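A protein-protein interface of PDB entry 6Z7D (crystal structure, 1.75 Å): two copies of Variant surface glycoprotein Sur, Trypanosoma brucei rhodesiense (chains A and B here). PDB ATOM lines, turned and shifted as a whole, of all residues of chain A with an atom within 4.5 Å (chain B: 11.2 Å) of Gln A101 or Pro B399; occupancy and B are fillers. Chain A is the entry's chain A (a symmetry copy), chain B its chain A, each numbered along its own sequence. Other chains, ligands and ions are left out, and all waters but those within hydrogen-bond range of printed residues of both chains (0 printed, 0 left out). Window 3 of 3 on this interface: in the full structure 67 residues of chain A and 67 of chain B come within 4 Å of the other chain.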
ATOM      1  N   ALA A  97      17.550   8.821   6.144  1.00  0.00           N
ATOM      2  CA  ALA A  97      18.932   9.233   5.908  1.00  0.00           C
ATOM      3  C   ALA A  97      19.190   9.440   4.424  1.00  0.00           C
ATOM      4  O   ALA A  97      19.795  10.440   4.014  1.00  0.00           O
ATOM      5  CB  ALA A  97      19.884   8.181   6.492  1.00  0.00           C
ATOM      6  N   TYR A  98      18.748   8.493   3.603  1.00  0.00           N
ATOM      7  CA  TYR A  98      18.863   8.635   2.155  1.00  0.00           C
ATOM      8  C   TYR A  98      18.182   9.915   1.675  1.00  0.00           C
ATOM      9  O   TYR A  98      18.767  10.703   0.929  1.00  0.00           O
ATOM     10  CB  TYR A  98      18.264   7.393   1.478  1.00  0.00           C
ATOM     11  CG  TYR A  98      18.198   7.498  -0.031  1.00  0.00           C
ATOM     12  CD1 TYR A  98      19.352   7.662  -0.777  1.00  0.00           C
ATOM     13  CD2 TYR A  98      16.984   7.454  -0.697  1.00  0.00           C
ATOM     14  CE1 TYR A  98      19.308   7.774  -2.161  1.00  0.00           C
ATOM     15  CE2 TYR A  98      16.925   7.576  -2.090  1.00  0.00           C
ATOM     16  CZ  TYR A  98      18.089   7.724  -2.808  1.00  0.00           C
ATOM     17  OH  TYR A  98      18.022   7.830  -4.179  1.00  0.00           O
ATOM     18  N   GLY A  99      16.950  10.158   2.121  1.00  0.00           N
ATOM     19  CA  GLY A  99      16.240  11.342   1.675  1.00  0.00           C
ATOM     20  C   GLY A  99      16.908  12.627   2.108  1.00  0.00           C
ATOM     21  O   GLY A  99      17.007  13.577   1.336  1.00  0.00           O
ATOM     22  N   ILE A 100      17.366  12.684   3.360  1.00  0.00           N
ATOM     23  CA  ILE A 100      18.040  13.892   3.810  1.00  0.00           C
ATOM     24  C   ILE A 100      19.286  14.133   2.966  1.00  0.00           C
ATOM     25  O   ILE A 100      19.517  15.241   2.470  1.00  0.00           O
ATOM     26  CB  ILE A 100      18.374  13.804   5.313  1.00  0.00           C
ATOM     27  CG1 ILE A 100      17.101  13.881   6.151  1.00  0.00           C
ATOM     28  CG2 ILE A 100      19.299  14.956   5.705  1.00  0.00           C
ATOM     29  CD1 ILE A 100      17.311  13.485   7.628  1.00  0.00           C
ATOM     30  N   GLN A 101      20.090  13.089   2.752  1.00  0.00           N
ATOM     31  CA  GLN A 101      21.316  13.274   1.986  1.00  0.00           C
ATOM     32  C   GLN A 101      21.030  13.833   0.606  1.00  0.00           C
ATOM     33  O   GLN A 101      21.585  14.874   0.209  1.00  0.00           O
ATOM     34  CB  GLN A 101      22.082  11.957   1.869  1.00  0.00           C
ATOM     35  CG  GLN A 101      23.411  12.126   1.161  1.00  0.00           C
ATOM     36  CD  GLN A 101      24.388  11.073   1.610  1.00  0.00           C
ATOM     37  OE1 GLN A 101      24.391   9.961   1.088  1.00  0.00           O
ATOM     38  NE2 GLN A 101      25.185  11.393   2.633  1.00  0.00           N
ATOM     39  N   ILE A 102      20.154  13.176  -0.152  1.00  0.00           N
ATOM     40  CA  ILE A 102      20.017  13.624  -1.535  1.00  0.00           C
ATOM     41  C   ILE A 102      19.289  14.966  -1.620  1.00  0.00           C
ATOM     42  O   ILE A 102      19.555  15.755  -2.533  1.00  0.00           O
ATOM     43  CB  ILE A 102      19.343  12.556  -2.420  1.00  0.00           C
ATOM     44  CG1 ILE A 102      17.873  12.366  -2.051  1.00  0.00           C
ATOM     45  CG2 ILE A 102      20.097  11.260  -2.287  1.00  0.00           C
ATOM     46  CD1 ILE A 102      17.099  11.497  -3.036  1.00  0.00           C
ATOM     47  N   THR A 103      18.409  15.278  -0.665  1.00  0.00           N
ATOM     48  CA  THR A 103      17.586  16.467  -0.828  1.00  0.00           C
ATOM     49  C   THR A 103      18.347  17.705  -0.381  1.00  0.00           C
ATOM     50  O   THR A 103      18.266  18.759  -1.031  1.00  0.00           O
ATOM     51  CB  THR A 103      16.260  16.311  -0.068  1.00  0.00           C
ATOM     52  OG1 THR A 103      15.638  15.065  -0.461  1.00  0.00           O
ATOM     53  CG2 THR A 103      15.292  17.454  -0.392  1.00  0.00           C
ATOM     54  N   VAL A 104      19.085  17.587   0.726  1.00  0.00           N
ATOM     55  CA  VAL A 104      19.951  18.674   1.175  1.00  0.00           C
ATOM     56  C   VAL A 104      20.996  18.961   0.107  1.00  0.00           C
ATOM     57  O   VAL A 104      21.241  20.119  -0.254  1.00  0.00           O
ATOM     58  CB  VAL A 104      20.609  18.322   2.528  1.00  0.00           C
ATOM     59  CG1 VAL A 104      21.676  19.350   2.880  1.00  0.00           C
ATOM     60  CG2 VAL A 104      19.571  18.242   3.674  1.00  0.00           C
ATOM     61  N   ASN A 105      21.607  17.906  -0.438  1.00  0.00           N
ATOM     62  CA  ASN A 105      22.590  18.095  -1.504  1.00  0.00           C
ATOM     63  C   ASN A 105      21.968  18.776  -2.712  1.00  0.00           C
ATOM     64  O   ASN A 105      22.564  19.688  -3.288  1.00  0.00           O
ATOM     65  CB  ASN A 105      23.203  16.759  -1.924  1.00  0.00           C
ATOM     66  CG  ASN A 105      24.220  16.914  -3.033  1.00  0.00           C
ATOM     67  OD1 ASN A 105      25.265  17.531  -2.850  1.00  0.00           O
ATOM     68  ND2 ASN A 105      23.924  16.349  -4.184  1.00  0.00           N
ATOM     69  N   GLU A 324      24.116   6.256  -2.885  1.00  0.00           N
ATOM     70  CA  GLU A 324      24.169   6.618  -1.468  1.00  0.00           C
ATOM     71  C   GLU A 324      23.734   5.495  -0.536  1.00  0.00           C
ATOM     72  O   GLU A 324      24.090   5.517   0.651  1.00  0.00           O
ATOM     73  CB  GLU A 324      23.284   7.841  -1.224  1.00  0.00           C
ATOM     74  CG  GLU A 324      23.752   9.091  -1.922  1.00  0.00           C
ATOM     75  CD  GLU A 324      23.217   9.260  -3.349  1.00  0.00           C
ATOM     76  OE1 GLU A 324      22.587   8.332  -3.929  1.00  0.00           O
ATOM     77  OE2 GLU A 324      23.449  10.358  -3.888  1.00  0.00           O
ATOM     78  N   ILE A 328      24.878   3.863   3.502  1.00  0.00           N
ATOM     79  CA  ILE A 328      23.782   3.954   4.462  1.00  0.00           C
ATOM     80  C   ILE A 328      23.363   2.563   4.908  1.00  0.00           C
ATOM     81  O   ILE A 328      23.323   2.264   6.108  1.00  0.00           O
ATOM     82  CB  ILE A 328      22.610   4.760   3.861  1.00  0.00           C
ATOM     83  CG1 ILE A 328      22.976   6.253   3.831  1.00  0.00           C
ATOM     84  CG2 ILE A 328      21.293   4.470   4.615  1.00  0.00           C
ATOM     85  CD1 ILE A 328      22.049   7.099   2.987  1.00  0.00           C
ATOM     86  N   ARG B  74      17.503  19.168  11.608  1.00  0.00           N
ATOM     87  CA  ARG B  74      18.437  18.113  11.224  1.00  0.00           C
ATOM     88  C   ARG B  74      19.545  17.941  12.270  1.00  0.00           C
ATOM     89  O   ARG B  74      20.002  16.821  12.504  1.00  0.00           O
ATOM     90  CB  ARG B  74      19.059  18.390   9.848  1.00  0.00           C
ATOM     91  CG  ARG B  74      18.074  18.347   8.667  1.00  0.00           C
ATOM     92  CD  ARG B  74      18.755  18.496   7.284  1.00  0.00           C
ATOM     93  NE  ARG B  74      19.432  19.778   7.029  1.00  0.00           N
ATOM     94  CZ  ARG B  74      18.865  20.903   6.589  1.00  0.00           C
ATOM     95  NH1 ARG B  74      17.566  20.972   6.317  1.00  0.00           N
ATOM     96  NH2 ARG B  74      19.627  21.982   6.389  1.00  0.00           N
ATOM     97  N   THR B  77      18.159  16.067  15.156  1.00  0.00           N
ATOM     98  CA  THR B  77      17.974  14.677  14.751  1.00  0.00           C
ATOM     99  C   THR B  77      19.264  13.890  14.911  1.00  0.00           C
ATOM    100  O   THR B  77      19.266  12.780  15.462  1.00  0.00           O
ATOM    101  CB  THR B  77      17.456  14.622  13.312  1.00  0.00           C
ATOM    102  OG1 THR B  77      16.223  15.322  13.249  1.00  0.00           O
ATOM    103  CG2 THR B  77      17.241  13.202  12.852  1.00  0.00           C
ATOM    104  N   LEU B  78      20.392  14.472  14.510  1.00  0.00           N
ATOM    105  CA  LEU B  78      21.658  13.777  14.718  1.00  0.00           C
ATOM    106  C   LEU B  78      21.957  13.593  16.215  1.00  0.00           C
ATOM    107  O   LEU B  78      22.307  12.487  16.667  1.00  0.00           O
ATOM    108  CB  LEU B  78      22.779  14.534  14.005  1.00  0.00           C
ATOM    109  CG  LEU B  78      24.140  13.857  14.193  1.00  0.00           C
ATOM    110  CD1 LEU B  78      24.092  12.399  13.736  1.00  0.00           C
ATOM    111  CD2 LEU B  78      25.234  14.604  13.467  1.00  0.00           C
ATOM    112  N   PHE B 381      33.788  10.374  11.817  1.00  0.00           N
ATOM    113  CA  PHE B 381      33.555   8.968  11.483  1.00  0.00           C
ATOM    114  C   PHE B 381      34.084   8.701  10.079  1.00  0.00           C
ATOM    115  O   PHE B 381      34.428   9.624   9.336  1.00  0.00           O
ATOM    116  CB  PHE B 381      32.071   8.596  11.569  1.00  0.00           C
ATOM    117  CG  PHE B 381      31.200   9.363  10.611  1.00  0.00           C
ATOM    118  CD1 PHE B 381      30.767   8.784   9.430  1.00  0.00           C
ATOM    119  CD2 PHE B 381      30.822  10.663  10.886  1.00  0.00           C
ATOM    120  CE1 PHE B 381      29.968   9.494   8.540  1.00  0.00           C
ATOM    121  CE2 PHE B 381      30.025  11.379   9.995  1.00  0.00           C
ATOM    122  CZ  PHE B 381      29.601  10.793   8.824  1.00  0.00           C
ATOM    123  N   SER B 389      34.617  14.292   9.549  1.00  0.00           N
ATOM    124  CA  SER B 389      34.789  15.250  10.643  1.00  0.00           C
ATOM    125  C   SER B 389      34.160  16.629  10.379  1.00  0.00           C
ATOM    126  O   SER B 389      34.525  17.321   9.428  1.00  0.00           O
ATOM    127  CB  SER B 389      36.274  15.422  10.947  1.00  0.00           C
ATOM    128  OG  SER B 389      36.476  16.388  11.964  1.00  0.00           O
ATOM    129  N   ASN B 390      33.222  17.032  11.233  1.00  0.00           N
ATOM    130  CA  ASN B 390      32.572  18.331  11.101  1.00  0.00           C
ATOM    131  C   ASN B 390      31.779  18.601  12.370  1.00  0.00           C
ATOM    132  O   ASN B 390      31.480  17.682  13.134  1.00  0.00           O
ATOM    133  CB  ASN B 390      31.647  18.372   9.885  1.00  0.00           C
ATOM    134  CG  ASN B 390      31.554  19.746   9.278  1.00  0.00           C
ATOM    135  OD1 ASN B 390      31.925  20.743   9.903  1.00  0.00           O
ATOM    136  ND2 ASN B 390      31.050  19.814   8.050  1.00  0.00           N
ATOM    137  N   THR B 391      31.429  19.867  12.583  1.00  0.00           N
ATOM    138  CA  THR B 391      30.539  20.181  13.689  1.00  0.00           C
ATOM    139  C   THR B 391      29.099  19.775  13.335  1.00  0.00           C
ATOM    140  O   THR B 391      28.749  19.596  12.167  1.00  0.00           O
ATOM    141  CB  THR B 391      30.629  21.668  14.042  1.00  0.00           C
ATOM    142  OG1 THR B 391      30.741  22.429  12.845  1.00  0.00           O
ATOM    143  CG2 THR B 391      31.857  21.942  14.879  1.00  0.00           C
ATOM    144  N   VAL B 392      28.266  19.632  14.372  1.00  0.00           N
ATOM    145  CA  VAL B 392      26.933  19.046  14.214  1.00  0.00           C
ATOM    146  C   VAL B 392      26.131  19.768  13.129  1.00  0.00           C
ATOM    147  O   VAL B 392      25.703  19.151  12.143  1.00  0.00           O
ATOM    148  CB  VAL B 392      26.184  19.046  15.557  1.00  0.00           C
ATOM    149  CG1 VAL B 392      24.734  18.584  15.369  1.00  0.00           C
ATOM    150  CG2 VAL B 392      26.901  18.133  16.542  1.00  0.00           C
ATOM    151  N   ALA B 393      25.906  21.081  13.298  1.00  0.00           N
ATOM    152  CA  ALA B 393      24.981  21.793  12.405  1.00  0.00           C
ATOM    153  C   ALA B 393      25.491  21.836  10.966  1.00  0.00           C
ATOM    154  O   ALA B 393      24.713  21.651  10.023  1.00  0.00           O
ATOM    155  CB  ALA B 393      24.711  23.211  12.913  1.00  0.00           C
ATOM    156  N   ALA B 394      26.791  22.077  10.774  1.00  0.00           N
ATOM    157  CA  ALA B 394      27.319  22.080   9.415  1.00  0.00           C
ATOM    158  C   ALA B 394      27.273  20.688   8.799  1.00  0.00           C
ATOM    159  O   ALA B 394      26.962  20.542   7.609  1.00  0.00           O
ATOM    160  CB  ALA B 394      28.745  22.628   9.396  1.00  0.00           C
ATOM    161  N   LEU B 395      27.576  19.653   9.594  1.00  0.00           N
ATOM    162  CA  LEU B 395      27.484  18.286   9.091  1.00  0.00           C
ATOM    163  C   LEU B 395      26.074  17.974   8.585  1.00  0.00           C
ATOM    164  O   LEU B 395      25.907  17.388   7.507  1.00  0.00           O
ATOM    165  CB  LEU B 395      27.908  17.305  10.188  1.00  0.00           C
ATOM    166  CG  LEU B 395      27.795  15.799   9.938  1.00  0.00           C
ATOM    167  CD1 LEU B 395      28.550  15.405   8.678  1.00  0.00           C
ATOM    168  CD2 LEU B 395      28.353  15.043  11.138  1.00  0.00           C
ATOM    169  N   MET B 396      25.043  18.360   9.344  1.00  0.00           N
ATOM    170  CA  MET B 396      23.689  17.980   8.973  1.00  0.00           C
ATOM    171  C   MET B 396      23.113  18.881   7.887  1.00  0.00           C
ATOM    172  O   MET B 396      21.958  18.693   7.487  1.00  0.00           O
ATOM    173  CB  MET B 396      22.778  17.971  10.202  1.00  0.00           C
ATOM    174  CG  MET B 396      23.129  16.832  11.204  1.00  0.00           C
ATOM    175  SD  MET B 396      23.291  15.271  10.292  1.00  0.00           S
ATOM    176  CE  MET B 396      21.591  14.999   9.805  1.00  0.00           C
ATOM    177  N   SER B 397      23.906  19.822   7.383  1.00  0.00           N
ATOM    178  CA  SER B 397      23.571  20.576   6.184  1.00  0.00           C
ATOM    179  C   SER B 397      24.547  20.288   5.053  1.00  0.00           C
ATOM    180  O   SER B 397      24.578  21.015   4.064  1.00  0.00           O
ATOM    181  CB  SER B 397      23.544  22.068   6.497  1.00  0.00           C
ATOM    182  OG  SER B 397      22.379  22.395   7.222  1.00  0.00           O
ATOM    183  N   SER B 398      25.336  19.241   5.175  1.00  0.00           N
ATOM    184  CA  SER B 398      26.414  18.930   4.259  1.00  0.00           C
ATOM    185  C   SER B 398      26.067  17.706   3.420  1.00  0.00           C
ATOM    186  O   SER B 398      25.054  17.041   3.658  1.00  0.00           O
ATOM    187  CB  SER B 398      27.696  18.673   5.056  1.00  0.00           C
ATOM    188  OG  SER B 398      27.705  17.330   5.497  1.00  0.00           O
ATOM    189  N   PRO B 399      26.895  17.379   2.419  1.00  0.00           N
ATOM    190  CA  PRO B 399      26.670  16.139   1.656  1.00  0.00           C
ATOM    191  C   PRO B 399      26.704  14.870   2.480  1.00  0.00           C
ATOM    192  O   PRO B 399      26.249  13.829   1.988  1.00  0.00           O
ATOM    193  CB  PRO B 399      27.811  16.151   0.631  1.00  0.00           C
ATOM    194  CG  PRO B 399      28.118  17.579   0.442  1.00  0.00           C
ATOM    195  CD  PRO B 399      27.907  18.235   1.769  1.00  0.00           C
ATOM    196  N   ASN B 400      27.234  14.904   3.702  1.00  0.00           N
ATOM    197  CA  ASN B 400      27.287  13.723   4.550  1.00  0.00           C
ATOM    198  C   ASN B 400      26.210  13.717   5.625  1.00  0.00           C
ATOM    199  O   ASN B 400      26.295  12.926   6.566  1.00  0.00           O
ATOM    200  CB  ASN B 400      28.667  13.597   5.193  1.00  0.00           C
ATOM    201  CG  ASN B 400      29.777  13.478   4.167  1.00  0.00           C
ATOM    202  OD1 ASN B 400      29.693  12.690   3.222  1.00  0.00           O
ATOM    203  ND2 ASN B 400      30.819  14.280   4.340  1.00  0.00           N
ATOM    204  N   SER B 401      25.192  14.567   5.503  1.00  0.00           N
ATOM    205  CA  SER B 401      24.179  14.664   6.542  1.00  0.00           C
ATOM    206  C   SER B 401      23.488  13.325   6.759  1.00  0.00           C
ATOM    207  O   SER B 401      23.517  12.757   7.859  1.00  0.00           O
ATOM    208  CB  SER B 401      23.168  15.729   6.141  1.00  0.00           C
ATOM    209  OG  SER B 401      22.705  15.428   4.836  1.00  0.00           O
ATOM    210  N   GLY B 402      22.858  12.802   5.711  1.00  0.00           N
ATOM    211  CA  GLY B 402      22.162  11.535   5.840  1.00  0.00           C
ATOM    212  C   GLY B 402      23.057  10.415   6.334  1.00  0.00           C
ATOM    213  O   GLY B 402      22.646   9.598   7.160  1.00  0.00           O
ATOM    214  N   LEU B 403      24.289  10.363   5.834  1.00  0.00           N
ATOM    215  CA  LEU B 403      25.204   9.285   6.190  1.00  0.00           C
ATOM    216  C   LEU B 403      25.634   9.367   7.655  1.00  0.00           C
ATOM    217  O   LEU B 403      25.841   8.333   8.310  1.00  0.00           O
ATOM    218  CB  LEU B 403      26.416   9.333   5.264  1.00  0.00           C
ATOM    219  CG  LEU B 403      27.518   8.321   5.526  1.00  0.00           C
ATOM    220  CD1 LEU B 403      26.942   6.922   5.363  1.00  0.00           C
ATOM    221  CD2 LEU B 403      28.685   8.558   4.577  1.00  0.00           C
ATOM    222  N   ALA B 404      25.788  10.587   8.181  1.00  0.00           N
ATOM    223  CA  ALA B 404      26.080  10.743   9.604  1.00  0.00           C
ATOM    224  C   ALA B 404      24.933  10.218  10.448  1.00  0.00           C
ATOM    225  O   ALA B 404      25.151   9.600  11.494  1.00  0.00           O
ATOM    226  CB  ALA B 404      26.350  12.209   9.947  1.00  0.00           C
ATOM    227  N   LEU B 405      23.701  10.454  10.005  1.00  0.00           N
ATOM    228  CA  LEU B 405      22.554   9.969  10.760  1.00  0.00           C
ATOM    229  C   LEU B 405      22.496   8.449  10.736  1.00  0.00           C
ATOM    230  O   LEU B 405      22.290   7.803  11.774  1.00  0.00           O
ATOM    231  CB  LEU B 405      21.279  10.581  10.184  1.00  0.00           C
ATOM    232  CG  LEU B 405      19.955  10.084  10.745  1.00  0.00           C
ATOM    233  CD1 LEU B 405      19.817  10.441  12.236  1.00  0.00           C
ATOM    234  CD2 LEU B 405      18.781  10.614   9.899  1.00  0.00           C
ATOM    235  N   ALA B 406      22.691   7.859   9.555  1.00  0.00           N
ATOM    236  CA  ALA B 406      22.657   6.398   9.443  1.00  0.00           C
ATOM    237  C   ALA B 406      23.754   5.763  10.277  1.00  0.00           C
ATOM    238  O   ALA B 406      23.526   4.773  10.985  1.00  0.00           O
ATOM    239  CB  ALA B 406      22.798   5.974   7.975  1.00  0.00           C
ATOM    240  N   TYR B 407      24.954   6.328  10.205  1.00  0.00           N
ATOM    241  CA  TYR B 407      26.076   5.790  10.958  1.00  0.00           C
ATOM    242  C   TYR B 407      25.794   5.784  12.458  1.00  0.00           C
ATOM    243  O   TYR B 407      26.085   4.799  13.143  1.00  0.00           O
ATOM    244  CB  TYR B 407      27.326   6.605  10.639  1.00  0.00           C
ATOM    245  CG  TYR B 407      28.542   6.186  11.417  1.00  0.00           C
ATOM    246  CD1 TYR B 407      29.324   5.124  10.997  1.00  0.00           C
ATOM    247  CD2 TYR B 407      28.907   6.854  12.577  1.00  0.00           C
ATOM    248  CE1 TYR B 407      30.435   4.735  11.706  1.00  0.00           C
ATOM    249  CE2 TYR B 407      30.025   6.471  13.303  1.00  0.00           C
ATOM    250  CZ  TYR B 407      30.793   5.409  12.865  1.00  0.00           C
ATOM    251  OH  TYR B 407      31.919   5.005  13.593  1.00  0.00           O
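Of the 11 printed residues of chain A, 5 touch a printed residue of chain B. Hydrophobic or aromatic side chains of chain A within 4 Å of the printed part of chain B: Ala A97, Ile A100, Val A104 and Ile A328. Hydrophobic or aromatic side chains of chain B that line the printed part of chain A: Leu B403, Leu B405 and Ala B406. Along chain B the printed residues that touch a printed residue of chain A span positions 74 to 406. Among the printed residues, 13 pairs touch across the chains. Among the printed residues, no Asp or Glu carboxylate lies within 4 Å of a Lys or Arg side-chain nitrogen of the other chain.
Ala A97 touches just these residues of chain B: Gly B402 and Ala B406. No residue of chain B comes within 4 Å of Gly A99. Of chain B, only Arg B74, Ser B401 and Leu B405 come within 4 Å of Ile A100. Of the printed residues of chain B, Gln A101 touches Pro B399, Asn B400, Ser B401, Gly B402 and Leu B403. No residue of chain B comes within 4 Å of Ile A102. Val A104 touches just these residues of chain B: Arg B74 (3.7 Å) and Ser B397 (3.5 Å). Ala B394 touches none of the printed residues of chain A. Met B396 touches none of the printed residues of chain A. Of the printed residues of chain A, Ser B397 touches Val A104 (3.5 Å). Printed residues of chain A within 4 Å of Pro B399: Gln A101. Of the printed residues of chain A, Asn B400 touches Gln A101. Of the printed residues of chain A, Ser B401 touches Ile A100 (3.5 Å) and Gln A101 (3.8 Å). Printed residues of chain A within 4 Å of Gly B402: Ala A97 and Gln A101. Printed residues of chain A within 4 Å of Leu B405: Ile A100.
No position is printed for both chains. Of the 13 pairs that touch across the chains among the printed residues, none has its exchanged pair printed and touching as well.
The backbone carbonyl oxygen (O) of Pro B399 is in hydrogen-bond range of the side-chain amide nitrogen (NE2) of Gln A101 (2.7 Å). The side-chain amide nitrogen (NE2) of Gln A101 sits close to the backbone NH (N) of Leu B403, at 3.5 Å.
OG of Ser B397 is in hydrogen-bond range of NH2 of Arg B74, at 2.9 Å. The side-chain hydroxyl (OG) of Ser B398 sits close to the backbone NH (N) of Asn B400 (3.1 Å). The side-chain hydroxyl (OG) of Ser B401 lies within hydrogen-bond range of the backbone carbonyl oxygen (O) of Ser B398, 3.1 Å away. The backbone carbonyl oxygen (O) of Met B396 is in hydrogen-bond range of the guanidinium group (NE) of Arg B74 (2.8 Å).
Among the printed residues, pairs that only touch across the chains: Ala A97 with Gly B402 (3.2 Å), Ile A100 with Ser B401 (3.5 Å), Val A104 with Ser B397 (3.5 Å), Gln A101 with Asn B400 (3.7 Å), Val A104 with Arg B74 (3.7 Å), Gln A101 with Ser B401 (3.8 Å), Ile A100 with Arg B74 (3.9 Å), Ile A100 with Leu B405 (3.9 Å), Ala A97 with Ala B406 (3.9 Å), Ile A328 with Ala B406 (3.98 Å) and Gln A101 with Gly B402 (3.99 Å).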
